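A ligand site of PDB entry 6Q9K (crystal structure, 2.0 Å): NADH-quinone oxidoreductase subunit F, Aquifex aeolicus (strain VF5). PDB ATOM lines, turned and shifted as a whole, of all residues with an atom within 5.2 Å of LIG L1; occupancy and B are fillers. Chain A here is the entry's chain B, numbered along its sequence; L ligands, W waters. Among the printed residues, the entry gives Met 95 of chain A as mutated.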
ATOM      1  N   GLY A  64      27.240   2.035 -14.301  1.00  0.00           N
ATOM      2  CA  GLY A  64      26.262   3.095 -13.975  1.00  0.00           C
ATOM      3  C   GLY A  64      26.761   4.028 -12.889  1.00  0.00           C
ATOM      4  O   GLY A  64      26.884   3.599 -11.706  1.00  0.00           O
ATOM      5  N   ARG A  65      27.000   5.284 -13.246  1.00  0.00           N
ATOM      6  CA  ARG A  65      27.538   6.339 -12.356  1.00  0.00           C
ATOM      7  C   ARG A  65      26.421   6.890 -11.463  1.00  0.00           C
ATOM      8  O   ARG A  65      26.717   7.744 -10.608  1.00  0.00           O
ATOM      9  CB  ARG A  65      28.215   7.414 -13.209  1.00  0.00           C
ATOM     10  CG  ARG A  65      29.332   6.899 -14.127  1.00  0.00           C
ATOM     11  CD  ARG A  65      30.491   6.289 -13.368  1.00  0.00           C
ATOM     12  NE  ARG A  65      31.744   6.296 -14.125  1.00  0.00           N
ATOM     13  CZ  ARG A  65      32.430   5.219 -14.509  1.00  0.00           C
ATOM     14  NH1 ARG A  65      33.565   5.375 -15.167  1.00  0.00           N
ATOM     15  NH2 ARG A  65      31.992   3.992 -14.254  1.00  0.00           N
ATOM     16  N   GLY A  66      25.166   6.440 -11.667  1.00  0.00           N
ATOM     17  CA  GLY A  66      24.008   6.812 -10.844  1.00  0.00           C
ATOM     18  C   GLY A  66      24.171   6.310  -9.417  1.00  0.00           C
ATOM     19  O   GLY A  66      23.582   6.924  -8.507  1.00  0.00           O
ATOM     20  N   GLY A  67      24.915   5.217  -9.216  1.00  0.00           N
ATOM     21  CA  GLY A  67      25.254   4.722  -7.867  1.00  0.00           C
ATOM     22  C   GLY A  67      25.223   3.210  -7.743  1.00  0.00           C
ATOM     23  O   GLY A  67      25.920   2.696  -6.841  1.00  0.00           O
ATOM     24  N   ALA A  68      24.435   2.505  -8.576  1.00  0.00           N
ATOM     25  CA  ALA A  68      24.312   1.029  -8.521  1.00  0.00           C
ATOM     26  C   ALA A  68      25.464   0.369  -9.277  1.00  0.00           C
ATOM     27  O   ALA A  68      25.733  -0.813  -8.992  1.00  0.00           O
ATOM     28  CB  ALA A  68      22.988   0.562  -9.063  1.00  0.00           C
ATOM     29  N   GLY A  69      26.098   1.075 -10.215  1.00  0.00           N
ATOM     30  CA  GLY A  69      27.240   0.550 -11.001  1.00  0.00           C
ATOM     31  C   GLY A  69      26.883  -0.638 -11.897  1.00  0.00           C
ATOM     32  O   GLY A  69      27.772  -1.470 -12.132  1.00  0.00           O
ATOM     33  N   PHE A  70      25.659  -0.699 -12.434  1.00  0.00           N
ATOM     34  CA  PHE A  70      25.270  -1.753 -13.406  1.00  0.00           C
ATOM     35  C   PHE A  70      26.028  -1.534 -14.726  1.00  0.00           C
ATOM     36  O   PHE A  70      26.132  -0.410 -15.200  1.00  0.00           O
ATOM     37  CB  PHE A  70      23.754  -1.764 -13.640  1.00  0.00           C
ATOM     38  CG  PHE A  70      23.277  -2.960 -14.406  1.00  0.00           C
ATOM     39  CD1 PHE A  70      22.925  -4.124 -13.754  1.00  0.00           C
ATOM     40  CD2 PHE A  70      23.208  -2.932 -15.792  1.00  0.00           C
ATOM     41  CE1 PHE A  70      22.496  -5.241 -14.467  1.00  0.00           C
ATOM     42  CE2 PHE A  70      22.766  -4.046 -16.499  1.00  0.00           C
ATOM     43  CZ  PHE A  70      22.414  -5.198 -15.839  1.00  0.00           C
ATOM     44  N   THR A  72      26.889  -0.708 -18.282  1.00  0.00           N
ATOM     45  CA  THR A  72      26.085   0.163 -19.176  1.00  0.00           C
ATOM     46  C   THR A  72      25.826  -0.557 -20.507  1.00  0.00           C
ATOM     47  O   THR A  72      24.666  -0.578 -20.949  1.00  0.00           O
ATOM     48  CB  THR A  72      26.758   1.527 -19.346  1.00  0.00           C
ATOM     49  OG1 THR A  72      27.029   2.066 -18.056  1.00  0.00           O
ATOM     50  CG2 THR A  72      25.902   2.483 -20.145  1.00  0.00           C
ATOM     51  N   LYS A  75      23.266  -3.260 -20.077  1.00  0.00           N
ATOM     52  CA  LYS A  75      21.898  -2.683 -19.987  1.00  0.00           C
ATOM     53  C   LYS A  75      21.374  -2.434 -21.410  1.00  0.00           C
ATOM     54  O   LYS A  75      20.247  -2.850 -21.697  1.00  0.00           O
ATOM     55  CB  LYS A  75      21.865  -1.385 -19.173  1.00  0.00           C
ATOM     56  CG  LYS A  75      20.457  -0.907 -18.834  1.00  0.00           C
ATOM     57  CD  LYS A  75      20.402   0.437 -18.155  1.00  0.00           C
ATOM     58  CE  LYS A  75      21.110   0.483 -16.819  1.00  0.00           C
ATOM     59  NZ  LYS A  75      20.953   1.811 -16.173  1.00  0.00           N
ATOM     60  N   ASN A  91      18.794  10.426 -16.576  1.00  0.00           N
ATOM     61  CA  ASN A  91      18.375  10.681 -15.181  1.00  0.00           C
ATOM     62  C   ASN A  91      19.227  11.819 -14.619  1.00  0.00           C
ATOM     63  O   ASN A  91      20.407  11.558 -14.329  1.00  0.00           O
ATOM     64  CB  ASN A  91      18.460   9.401 -14.340  1.00  0.00           C
ATOM     65  CG  ASN A  91      17.815   9.584 -12.984  1.00  0.00           C
ATOM     66  OD1 ASN A  91      17.603  10.713 -12.550  1.00  0.00           O
ATOM     67  ND2 ASN A  91      17.466   8.482 -12.332  1.00  0.00           N
ATOM     68  N   ASP A  93      17.994  13.690 -11.912  1.00  0.00           N
ATOM     69  CA  ASP A  93      17.228  13.986 -10.671  1.00  0.00           C
ATOM     70  C   ASP A  93      18.171  14.325  -9.522  1.00  0.00           C
ATOM     71  O   ASP A  93      17.731  15.068  -8.644  1.00  0.00           O
ATOM     72  CB  ASP A  93      16.261  12.862 -10.298  1.00  0.00           C
ATOM     73  CG  ASP A  93      15.163  13.389  -9.419  1.00  0.00           C
ATOM     74  OD1 ASP A  93      14.447  14.313  -9.865  1.00  0.00           O
ATOM     75  OD2 ASP A  93      15.070  12.918  -8.255  1.00  0.00           O
ATOM     76  N   GLU A  94      19.394  13.774  -9.503  1.00  0.00           N
ATOM     77  CA  GLU A  94      20.439  13.964  -8.455  1.00  0.00           C
ATOM     78  C   GLU A  94      19.887  14.610  -7.181  1.00  0.00           C
ATOM     79  O   GLU A  94      19.959  15.850  -7.041  1.00  0.00           O
ATOM     80  CB  GLU A  94      21.574  14.819  -9.032  1.00  0.00           C
ATOM     81  CG  GLU A  94      22.687  15.042  -8.034  1.00  0.00           C
ATOM     82  CD  GLU A  94      23.952  15.576  -8.670  1.00  0.00           C
ATOM     83  OE1 GLU A  94      23.949  16.750  -9.077  1.00  0.00           O
ATOM     84  OE2 GLU A  94      24.909  14.787  -8.802  1.00  0.00           O
ATOM     85  N   MET A  95      19.381  13.808  -6.233  1.00  0.00           N
ATOM     86  CA  MET A  95      18.813  14.336  -4.968  1.00  0.00           C
ATOM     87  C   MET A  95      19.342  13.571  -3.741  1.00  0.00           C
ATOM     88  O   MET A  95      18.814  13.819  -2.654  1.00  0.00           O
ATOM     89  CB  MET A  95      17.282  14.290  -4.977  1.00  0.00           C
ATOM     90  CG  MET A  95      16.691  15.450  -5.744  1.00  0.00           C
ATOM     91  SD  MET A  95      14.910  15.423  -5.858  1.00  0.00           S
ATOM     92  CE  MET A  95      14.449  15.898  -4.192  1.00  0.00           C
ATOM     93  N   ASP A 102      26.554  15.611 -10.857  1.00  0.00           N
ATOM     94  CA  ASP A 102      25.894  15.666 -12.195  1.00  0.00           C
ATOM     95  C   ASP A 102      25.658  17.118 -12.616  1.00  0.00           C
ATOM     96  O   ASP A 102      25.785  17.422 -13.837  1.00  0.00           O
ATOM     97  CB  ASP A 102      24.553  14.911 -12.196  1.00  0.00           C
ATOM     98  CG  ASP A 102      24.674  13.423 -11.914  1.00  0.00           C
ATOM     99  OD1 ASP A 102      25.810  12.889 -12.044  1.00  0.00           O
ATOM    100  OD2 ASP A 102      23.654  12.797 -11.565  1.00  0.00           O
ATOM    101  N   TYR A 179      12.503  13.066  -4.172  1.00  0.00           N
ATOM    102  CA  TYR A 179      13.714  12.212  -4.234  1.00  0.00           C
ATOM    103  C   TYR A 179      13.400  10.919  -4.998  1.00  0.00           C
ATOM    104  O   TYR A 179      14.232  10.459  -5.799  1.00  0.00           O
ATOM    105  CB  TYR A 179      14.168  11.907  -2.800  1.00  0.00           C
ATOM    106  CG  TYR A 179      15.200  10.831  -2.599  1.00  0.00           C
ATOM    107  CD1 TYR A 179      16.523  11.021  -2.955  1.00  0.00           C
ATOM    108  CD2 TYR A 179      14.881   9.664  -1.928  1.00  0.00           C
ATOM    109  CE1 TYR A 179      17.476  10.059  -2.689  1.00  0.00           C
ATOM    110  CE2 TYR A 179      15.819   8.693  -1.652  1.00  0.00           C
ATOM    111  CZ  TYR A 179      17.136   8.892  -2.043  1.00  0.00           C
ATOM    112  OH  TYR A 179      18.074   7.944  -1.750  1.00  0.00           O
ATOM    113  N   ILE A 180      12.223  10.349  -4.712  1.00  0.00           N
ATOM    114  CA  ILE A 180      11.797   9.030  -5.259  1.00  0.00           C
ATOM    115  C   ILE A 180      11.730   9.108  -6.784  1.00  0.00           C
ATOM    116  O   ILE A 180      11.829   8.052  -7.408  1.00  0.00           O
ATOM    117  CB  ILE A 180      10.464   8.571  -4.648  1.00  0.00           C
ATOM    118  CG1 ILE A 180      10.193   7.088  -4.950  1.00  0.00           C
ATOM    119  CG2 ILE A 180       9.302   9.449  -5.102  1.00  0.00           C
ATOM    120  CD1 ILE A 180      11.304   6.166  -4.488  1.00  0.00           C
ATOM    121  N   GLY A 182      13.831  10.077  -8.774  1.00  0.00           N
ATOM    122  CA  GLY A 182      15.130   9.615  -9.310  1.00  0.00           C
ATOM    123  C   GLY A 182      15.166   8.112  -9.491  1.00  0.00           C
ATOM    124  O   GLY A 182      15.995   7.638 -10.272  1.00  0.00           O
ATOM    125  N   GLU A 183      14.324   7.359  -8.766  1.00  0.00           N
ATOM    126  CA  GLU A 183      14.173   5.904  -9.002  1.00  0.00           C
ATOM    127  C   GLU A 183      13.605   5.746 -10.414  1.00  0.00           C
ATOM    128  O   GLU A 183      12.599   6.402 -10.723  1.00  0.00           O
ATOM    129  CB  GLU A 183      13.321   5.249  -7.921  1.00  0.00           C
ATOM    130  CG  GLU A 183      13.504   3.742  -7.847  1.00  0.00           C
ATOM    131  CD  GLU A 183      12.657   2.918  -8.798  1.00  0.00           C
ATOM    132  OE1 GLU A 183      11.779   3.493  -9.499  1.00  0.00           O
ATOM    133  OE2 GLU A 183      12.854   1.693  -8.819  1.00  0.00           O
ATOM    134  N   GLU A 184      14.270   4.944 -11.253  1.00  0.00           N
ATOM    135  CA  GLU A 184      14.053   4.926 -12.720  1.00  0.00           C
ATOM    136  C   GLU A 184      12.581   4.671 -13.061  1.00  0.00           C
ATOM    137  O   GLU A 184      12.105   5.278 -14.023  1.00  0.00           O
ATOM    138  CB  GLU A 184      14.956   3.882 -13.382  1.00  0.00           C
ATOM    139  CG  GLU A 184      14.827   2.482 -12.821  1.00  0.00           C
ATOM    140  CD  GLU A 184      15.680   1.466 -13.560  1.00  0.00           C
ATOM    141  OE1 GLU A 184      16.458   1.896 -14.448  1.00  0.00           O
ATOM    142  OE2 GLU A 184      15.568   0.268 -13.247  1.00  0.00           O
ATOM    143  N   VAL A 217      17.304   3.844 -18.938  1.00  0.00           N
ATOM    144  CA  VAL A 217      17.552   4.976 -18.009  1.00  0.00           C
ATOM    145  C   VAL A 217      19.034   4.941 -17.657  1.00  0.00           C
ATOM    146  O   VAL A 217      19.492   3.889 -17.189  1.00  0.00           O
ATOM    147  CB  VAL A 217      16.673   4.917 -16.749  1.00  0.00           C
ATOM    148  CG1 VAL A 217      16.936   6.129 -15.844  1.00  0.00           C
ATOM    149  CG2 VAL A 217      15.189   4.820 -17.102  1.00  0.00           C
ATOM    150  N   ASN A 218      19.746   6.033 -17.910  1.00  0.00           N
ATOM    151  CA  ASN A 218      21.163   6.193 -17.481  1.00  0.00           C
ATOM    152  C   ASN A 218      21.336   7.564 -16.833  1.00  0.00           C
ATOM    153  O   ASN A 218      20.611   8.504 -17.171  1.00  0.00           O
ATOM    154  CB  ASN A 218      22.161   6.007 -18.627  1.00  0.00           C
ATOM    155  CG  ASN A 218      22.493   4.562 -18.911  1.00  0.00           C
ATOM    156  OD1 ASN A 218      22.336   4.106 -20.043  1.00  0.00           O
ATOM    157  ND2 ASN A 218      22.997   3.843 -17.913  1.00  0.00           N
ATOM    158  N   ASN A 219      22.266   7.600 -15.894  1.00  0.00           N
ATOM    159  CA  ASN A 219      22.688   8.784 -15.117  1.00  0.00           C
ATOM    160  C   ASN A 219      23.473   9.727 -16.032  1.00  0.00           C
ATOM    161  O   ASN A 219      24.174   9.232 -16.938  1.00  0.00           O
ATOM    162  CB  ASN A 219      23.515   8.302 -13.915  1.00  0.00           C
ATOM    163  CG  ASN A 219      24.174   9.424 -13.142  1.00  0.00           C
ATOM    164  OD1 ASN A 219      25.379   9.632 -13.270  1.00  0.00           O
ATOM    165  ND2 ASN A 219      23.381  10.122 -12.351  1.00  0.00           N
ATOM    166  N   VAL A 220      23.359  11.026 -15.772  1.00  0.00           N
ATOM    167  CA  VAL A 220      24.114  12.137 -16.405  1.00  0.00           C
ATOM    168  C   VAL A 220      25.588  11.735 -16.580  1.00  0.00           C
ATOM    169  O   VAL A 220      26.108  11.790 -17.720  1.00  0.00           O
ATOM    170  CB  VAL A 220      23.968  13.422 -15.546  1.00  0.00           C
ATOM    171  CG1 VAL A 220      25.011  14.476 -15.878  1.00  0.00           C
ATOM    172  CG2 VAL A 220      22.573  14.007 -15.647  1.00  0.00           C
ATOM    173  N   THR A 222      27.205   8.839 -16.339  1.00  0.00           N
ATOM    174  CA  THR A 222      27.342   7.643 -17.211  1.00  0.00           C
ATOM    175  C   THR A 222      27.394   8.103 -18.672  1.00  0.00           C
ATOM    176  O   THR A 222      28.353   7.758 -19.380  1.00  0.00           O
ATOM    177  CB  THR A 222      26.206   6.625 -16.984  1.00  0.00           C
ATOM    178  OG1 THR A 222      26.112   6.352 -15.588  1.00  0.00           O
ATOM    179  CG2 THR A 222      26.426   5.339 -17.752  1.00  0.00           C
ATOM    180  N   CYS A 392      11.208  -0.989  -4.150  1.00  0.00           N
ATOM    181  CA  CYS A 392      12.343  -0.170  -4.667  1.00  0.00           C
ATOM    182  C   CYS A 392      13.445  -0.003  -3.619  1.00  0.00           C
ATOM    183  O   CYS A 392      13.250  -0.385  -2.440  1.00  0.00           O
ATOM    184  CB  CYS A 392      11.856   1.183  -5.199  1.00  0.00           C
ATOM    185  SG  CYS A 392      11.908   2.519  -3.990  1.00  0.00           S
ATOM    186  N   GLY A 393      14.574   0.550  -4.052  1.00  0.00           N
ATOM    187  CA  GLY A 393      15.809   0.675  -3.268  1.00  0.00           C
ATOM    188  C   GLY A 393      15.664   1.555  -2.029  1.00  0.00           C
ATOM    189  O   GLY A 393      16.502   1.403  -1.141  1.00  0.00           O
ATOM    190  N   LEU A 394      14.687   2.474  -1.979  1.00  0.00           N
ATOM    191  CA  LEU A 394      14.527   3.416  -0.837  1.00  0.00           C
ATOM    192  C   LEU A 394      14.187   2.598   0.419  1.00  0.00           C
ATOM    193  O   LEU A 394      14.930   2.705   1.415  1.00  0.00           O
ATOM    194  CB  LEU A 394      13.443   4.461  -1.129  1.00  0.00           C
ATOM    195  CG  LEU A 394      13.416   5.654  -0.174  1.00  0.00           C
ATOM    196  CD1 LEU A 394      12.761   6.867  -0.815  1.00  0.00           C
ATOM    197  CD2 LEU A 394      12.709   5.301   1.139  1.00  0.00           C
HETATM  198  N1  LIG L   1      19.920   7.449 -10.344  1.00  0.00           N
HETATM  199  C1  LIG L   1      20.296   8.651 -10.879  1.00  0.00           C
HETATM  200  O1  LIG L   1      20.986   8.707 -11.911  1.00  0.00           O
HETATM  201  N2  LIG L   1      19.856   9.835 -10.275  1.00  0.00           N
HETATM  202  C2  LIG L   1      19.013   9.931  -9.186  1.00  0.00           C
HETATM  203  O2  LIG L   1      18.700  11.031  -8.744  1.00  0.00           O
HETATM  204  C3  LIG L   1      18.590   8.628  -8.649  1.00  0.00           C
HETATM  205  N3  LIG L   1      17.743   8.616  -7.652  1.00  0.00           N
HETATM  206  C4  LIG L   1      17.330   7.379  -7.156  1.00  0.00           C
HETATM  207  C5  LIG L   1      16.452   7.345  -6.073  1.00  0.00           C
HETATM  208  C6  LIG L   1      16.068   6.139  -5.497  1.00  0.00           C
HETATM  209  C7  LIG L   1      15.134   6.140  -4.311  1.00  0.00           C
HETATM  210  C8  LIG L   1      16.566   4.931  -6.029  1.00  0.00           C
HETATM  211  C9  LIG L   1      16.236   3.604  -5.392  1.00  0.00           C
HETATM  212  C10 LIG L   1      17.401   4.961  -7.134  1.00  0.00           C
HETATM  213  C11 LIG L   1      17.806   6.170  -7.699  1.00  0.00           C
HETATM  214  N4  LIG L   1      18.702   6.238  -8.804  1.00  0.00           N
HETATM  215  C12 LIG L   1      19.102   7.455  -9.297  1.00  0.00           C
HETATM  216  C13 LIG L   1      19.141   5.031  -9.519  1.00  0.00           C
HETATM  217  C14 LIG L   1      18.257   4.742 -10.731  1.00  0.00           C
HETATM  218  O3  LIG L   1      17.095   4.015 -10.339  1.00  0.00           O
HETATM  219  C15 LIG L   1      19.036   3.955 -11.796  1.00  0.00           C
HETATM  220  O4  LIG L   1      19.721   2.880 -11.184  1.00  0.00           O
HETATM  221  C16 LIG L   1      20.046   4.779 -12.592  1.00  0.00           C
HETATM  222  O5  LIG L   1      19.493   6.042 -12.973  1.00  0.00           O
HETATM  223  C17 LIG L   1      20.511   4.020 -13.814  1.00  0.00           C
HETATM  224  O6  LIG L   1      21.576   4.758 -14.431  1.00  0.00           O
HETATM  225  P1  LIG L   1      23.082   4.256 -14.338  1.00  0.00           P
HETATM  226  O7  LIG L   1      23.622   4.526 -12.961  1.00  0.00           O
HETATM  227  O8  LIG L   1      23.085   2.745 -14.677  1.00  0.00           O
HETATM  228  O9  LIG L   1      23.801   4.982 -15.476  1.00  0.00           O
HETATM  229  P1  LG2 L   2      19.664  -1.613  -9.191  1.00  0.00           P
HETATM  230  O1  LG2 L   2      20.971  -2.221  -8.841  1.00  0.00           O
HETATM  231  O2  LG2 L   2      18.451  -2.420  -8.874  1.00  0.00           O
HETATM  232  O3  LG2 L   2      19.583  -1.295 -10.792  1.00  0.00           O
HETATM  233  C1  LG2 L   2      20.629  -0.532 -11.431  1.00  0.00           C
HETATM  234  C2  LG2 L   2      20.327  -0.391 -12.894  1.00  0.00           C
HETATM  235  O4  LG2 L   2      20.557  -1.672 -13.537  1.00  0.00           O
HETATM  236  C3  LG2 L   2      18.899   0.022 -13.252  1.00  0.00           C
HETATM  237  O5  LG2 L   2      18.853   0.867 -14.396  1.00  0.00           O
HETATM  238  C4  LG2 L   2      18.216  -1.320 -13.527  1.00  0.00           C
HETATM  239  O6  LG2 L   2      17.141  -1.188 -14.443  1.00  0.00           O
HETATM  240  C5  LG2 L   2      19.363  -2.127 -14.157  1.00  0.00           C
HETATM  241  N1  LG2 L   2      19.245  -3.564 -13.938  1.00  0.00           N
HETATM  242  C6  LG2 L   2      19.462  -4.254 -12.776  1.00  0.00           C
HETATM  243  N2  LG2 L   2      19.238  -5.544 -12.860  1.00  0.00           N
HETATM  244  C7  LG2 L   2      18.829  -5.720 -14.176  1.00  0.00           C
HETATM  245  C8  LG2 L   2      18.420  -6.849 -14.908  1.00  0.00           C
HETATM  246  N3  LG2 L   2      18.318  -8.079 -14.374  1.00  0.00           N
HETATM  247  N4  LG2 L   2      18.083  -6.672 -16.207  1.00  0.00           N
HETATM  248  C9  LG2 L   2      18.159  -5.447 -16.724  1.00  0.00           C
HETATM  249  N5  LG2 L   2      18.523  -4.299 -16.142  1.00  0.00           N
HETATM  250  C10 LG2 L   2      18.843  -4.510 -14.857  1.00  0.00           C
HETATM  251  O7  LG2 L   2      19.518  -0.220  -8.443  1.00  0.00           O
HETATM  252  P2  LG2 L   2      18.486   0.984  -8.340  1.00  0.00           P
HETATM  253  O8  LG2 L   2      17.490   0.639  -7.262  1.00  0.00           O
HETATM  254  O9  LG2 L   2      17.958   1.430  -9.661  1.00  0.00           O
HETATM  255  O10 LG2 L   2      19.476   2.102  -7.728  1.00  0.00           O
HETATM  256  C11 LG2 L   2      20.054   2.101  -6.398  1.00  0.00           C
HETATM  257  C12 LG2 L   2      21.119   3.166  -6.349  1.00  0.00           C
HETATM  258  O11 LG2 L   2      20.535   4.467  -6.521  1.00  0.00           O
HETATM  259  C13 LG2 L   2      21.890   3.253  -5.027  1.00  0.00           C
HETATM  260  O12 LG2 L   2      23.075   2.477  -5.113  1.00  0.00           O
HETATM  261  C14 LG2 L   2      22.192   4.756  -4.869  1.00  0.00           C
HETATM  262  O13 LG2 L   2      23.597   4.984  -4.889  1.00  0.00           O
HETATM  263  C15 LG2 L   2      21.527   5.387  -6.105  1.00  0.00           C
HETATM  264  N6  LG2 L   2      20.907   6.686  -5.872  1.00  0.00           N
HETATM  265  C16 LG2 L   2      21.433   7.865  -6.471  1.00  0.00           C
HETATM  266  C17 LG2 L   2      20.900   9.088  -6.261  1.00  0.00           C
HETATM  267  C18 LG2 L   2      21.558  10.256  -6.883  1.00  0.00           C
HETATM  268  O14 LG2 L   2      21.273  11.398  -6.496  1.00  0.00           O
HETATM  269  N7  LG2 L   2      22.451  10.049  -7.854  1.00  0.00           N
HETATM  270  C19 LG2 L   2      19.725   9.259  -5.370  1.00  0.00           C
HETATM  271  C20 LG2 L   2      19.235   7.961  -4.822  1.00  0.00           C
HETATM  272  C21 LG2 L   2      19.813   6.802  -5.068  1.00  0.00           C
HETATM  273  O   HOH W   1      24.665   1.655 -16.471  1.00  0.00           O
HETATM  274  O   HOH W   2      16.798  11.395  -6.755  1.00  0.00           O
HETATM  275  O   HOH W   3      23.575   1.296 -12.517  1.00  0.00           O
HETATM  276  O   HOH W   4      22.613   3.324 -10.858  1.00  0.00           O
HETATM  277  O   HOH W   5      21.051  12.237 -11.545  1.00  0.00           O
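Water W4 lies within hydrogen-bond range of an oxygen (O7) of LIG L1 (2.6 Å), the backbone NH of Ala 68 (3.0 Å) and the backbone NH of Gly 67 (3.4 Å).
Water W1 lies within hydrogen-bond range of an oxygen (O8) of LIG L1, the backbone carbonyl oxygen (O) of Phe 70, the side-chain hydroxyl (OG1) of Thr 72, the side-chain amide nitrogen (ND2) of Asn 218 and the backbone NH (N) of Gly 64.
Water W3 lies within hydrogen-bond range of O8 of LIG L1 (2.6 Å), N of Phe 70 (2.9 Å) and N of Gly 69 (3.4 Å).
O9 of LG2 L2 lies within hydrogen-bond range of O4 of LIG L1 (2.7 Å).
The backbone carbonyl oxygen (O) of Gly 182 lies close to a nitrogen (N3) of LIG L1.
Gly 64 touches LIG L1 (CA to O7, 3.2 Å).
Asp 93 touches LIG L1.
N of Met 95 touches O2 of LIG L1 (3.8 Å).
Tyr 179 touches LIG L1 (CE2 to C7, 3.7 Å).
CD1 of Ile 180 touches C7 of LIG L1, at 3.8 Å.
N of Glu 183 touches C4 of LIG L1, 3.4 Å away.
Val 217 touches LIG L1 (O to C17, 3.5 Å).
CA of Gly 393 touches C9 of LIG L1, at 3.6 Å.
N of Leu 394 touches C9 of LIG L1, at 3.9 Å.
Hydrophobic or aromatic side chains within 4 Å of LIG L1: Tyr 179, Ile 180, Val 217 and Leu 394.
O9 of LIG L1 is in hydrogen-bond range of N of Asn 219 (3.1 Å).
The backbone carbonyl oxygen (O) of Gly 66 sits close to a nitrogen (N7) of LG2 L2.
The side-chain amide nitrogen of Asn 218 lies within hydrogen-bond range of an oxygen (O9) of LIG L1 (2.8 Å).
The side-chain amide nitrogen (ND2) of Asn 91 sits close to an oxygen (O5) of LIG L1 (3.2 Å).
OG1 of Thr 222 sits at hydrogen-bond distance from O9 of LIG L1 (2.7 Å).
N of Gly 66 is in hydrogen-bond range of O7 of LIG L1 (2.8 Å).
O6 of LG2 L2 is in hydrogen-bond range of OE2 of Glu 184, 2.5 Å away.
The backbone NH of Glu 94 lies within hydrogen-bond range of an oxygen (O2) of LIG L1, at 2.9 Å.
NZ of Lys 75 lies within salt-bridge range of O8 of LIG L1, at 2.8 Å.
The side-chain amino group (NZ) of Lys 75 sits at hydrogen-bond distance from an oxygen (O5) of LG2 L2.
An oxygen (O14) of LG2 L2 is in hydrogen-bond range of the backbone NH (N) of Met 95.
N of Glu 184 sits at hydrogen-bond distance from O3 of LIG L1, 3.1 Å away.
O12 of LG2 L2 is in hydrogen-bond range of O of Gly 67.
The side-chain amide nitrogen (ND2) of Asn 219 sits at hydrogen-bond distance from an oxygen (O1) of LIG L1 (2.8 Å).
N of Arg 65 is in hydrogen-bond range of O7 of LIG L1, 3.5 Å away.
The backbone NH of Asp 93 lies within hydrogen-bond range of the side-chain amide oxygen of Asn 91.
NZ of Lys 75 sits at hydrogen-bond distance from O of Val 217 (2.7 Å).
The side-chain carboxylate of Glu 94 lies within hydrogen-bond range of the backbone NH of Asp 102 (2.8 Å).
The backbone NH (N) of Gly 69 lies within hydrogen-bond range of the backbone carbonyl oxygen (O) of Gly 64 (3.0 Å).
OG1 of Thr 222 lies within hydrogen-bond range of N of Arg 65 (2.7 Å).
OD2 of Asp 93 lies within hydrogen-bond range of N of Gly 182, 3.1 Å away.
The backbone carbonyl oxygen of Phe 70 lies within hydrogen-bond range of the backbone NH of Gly 64.
N of Tyr 179 sits close to SD of Met 95, 3.8 Å away.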
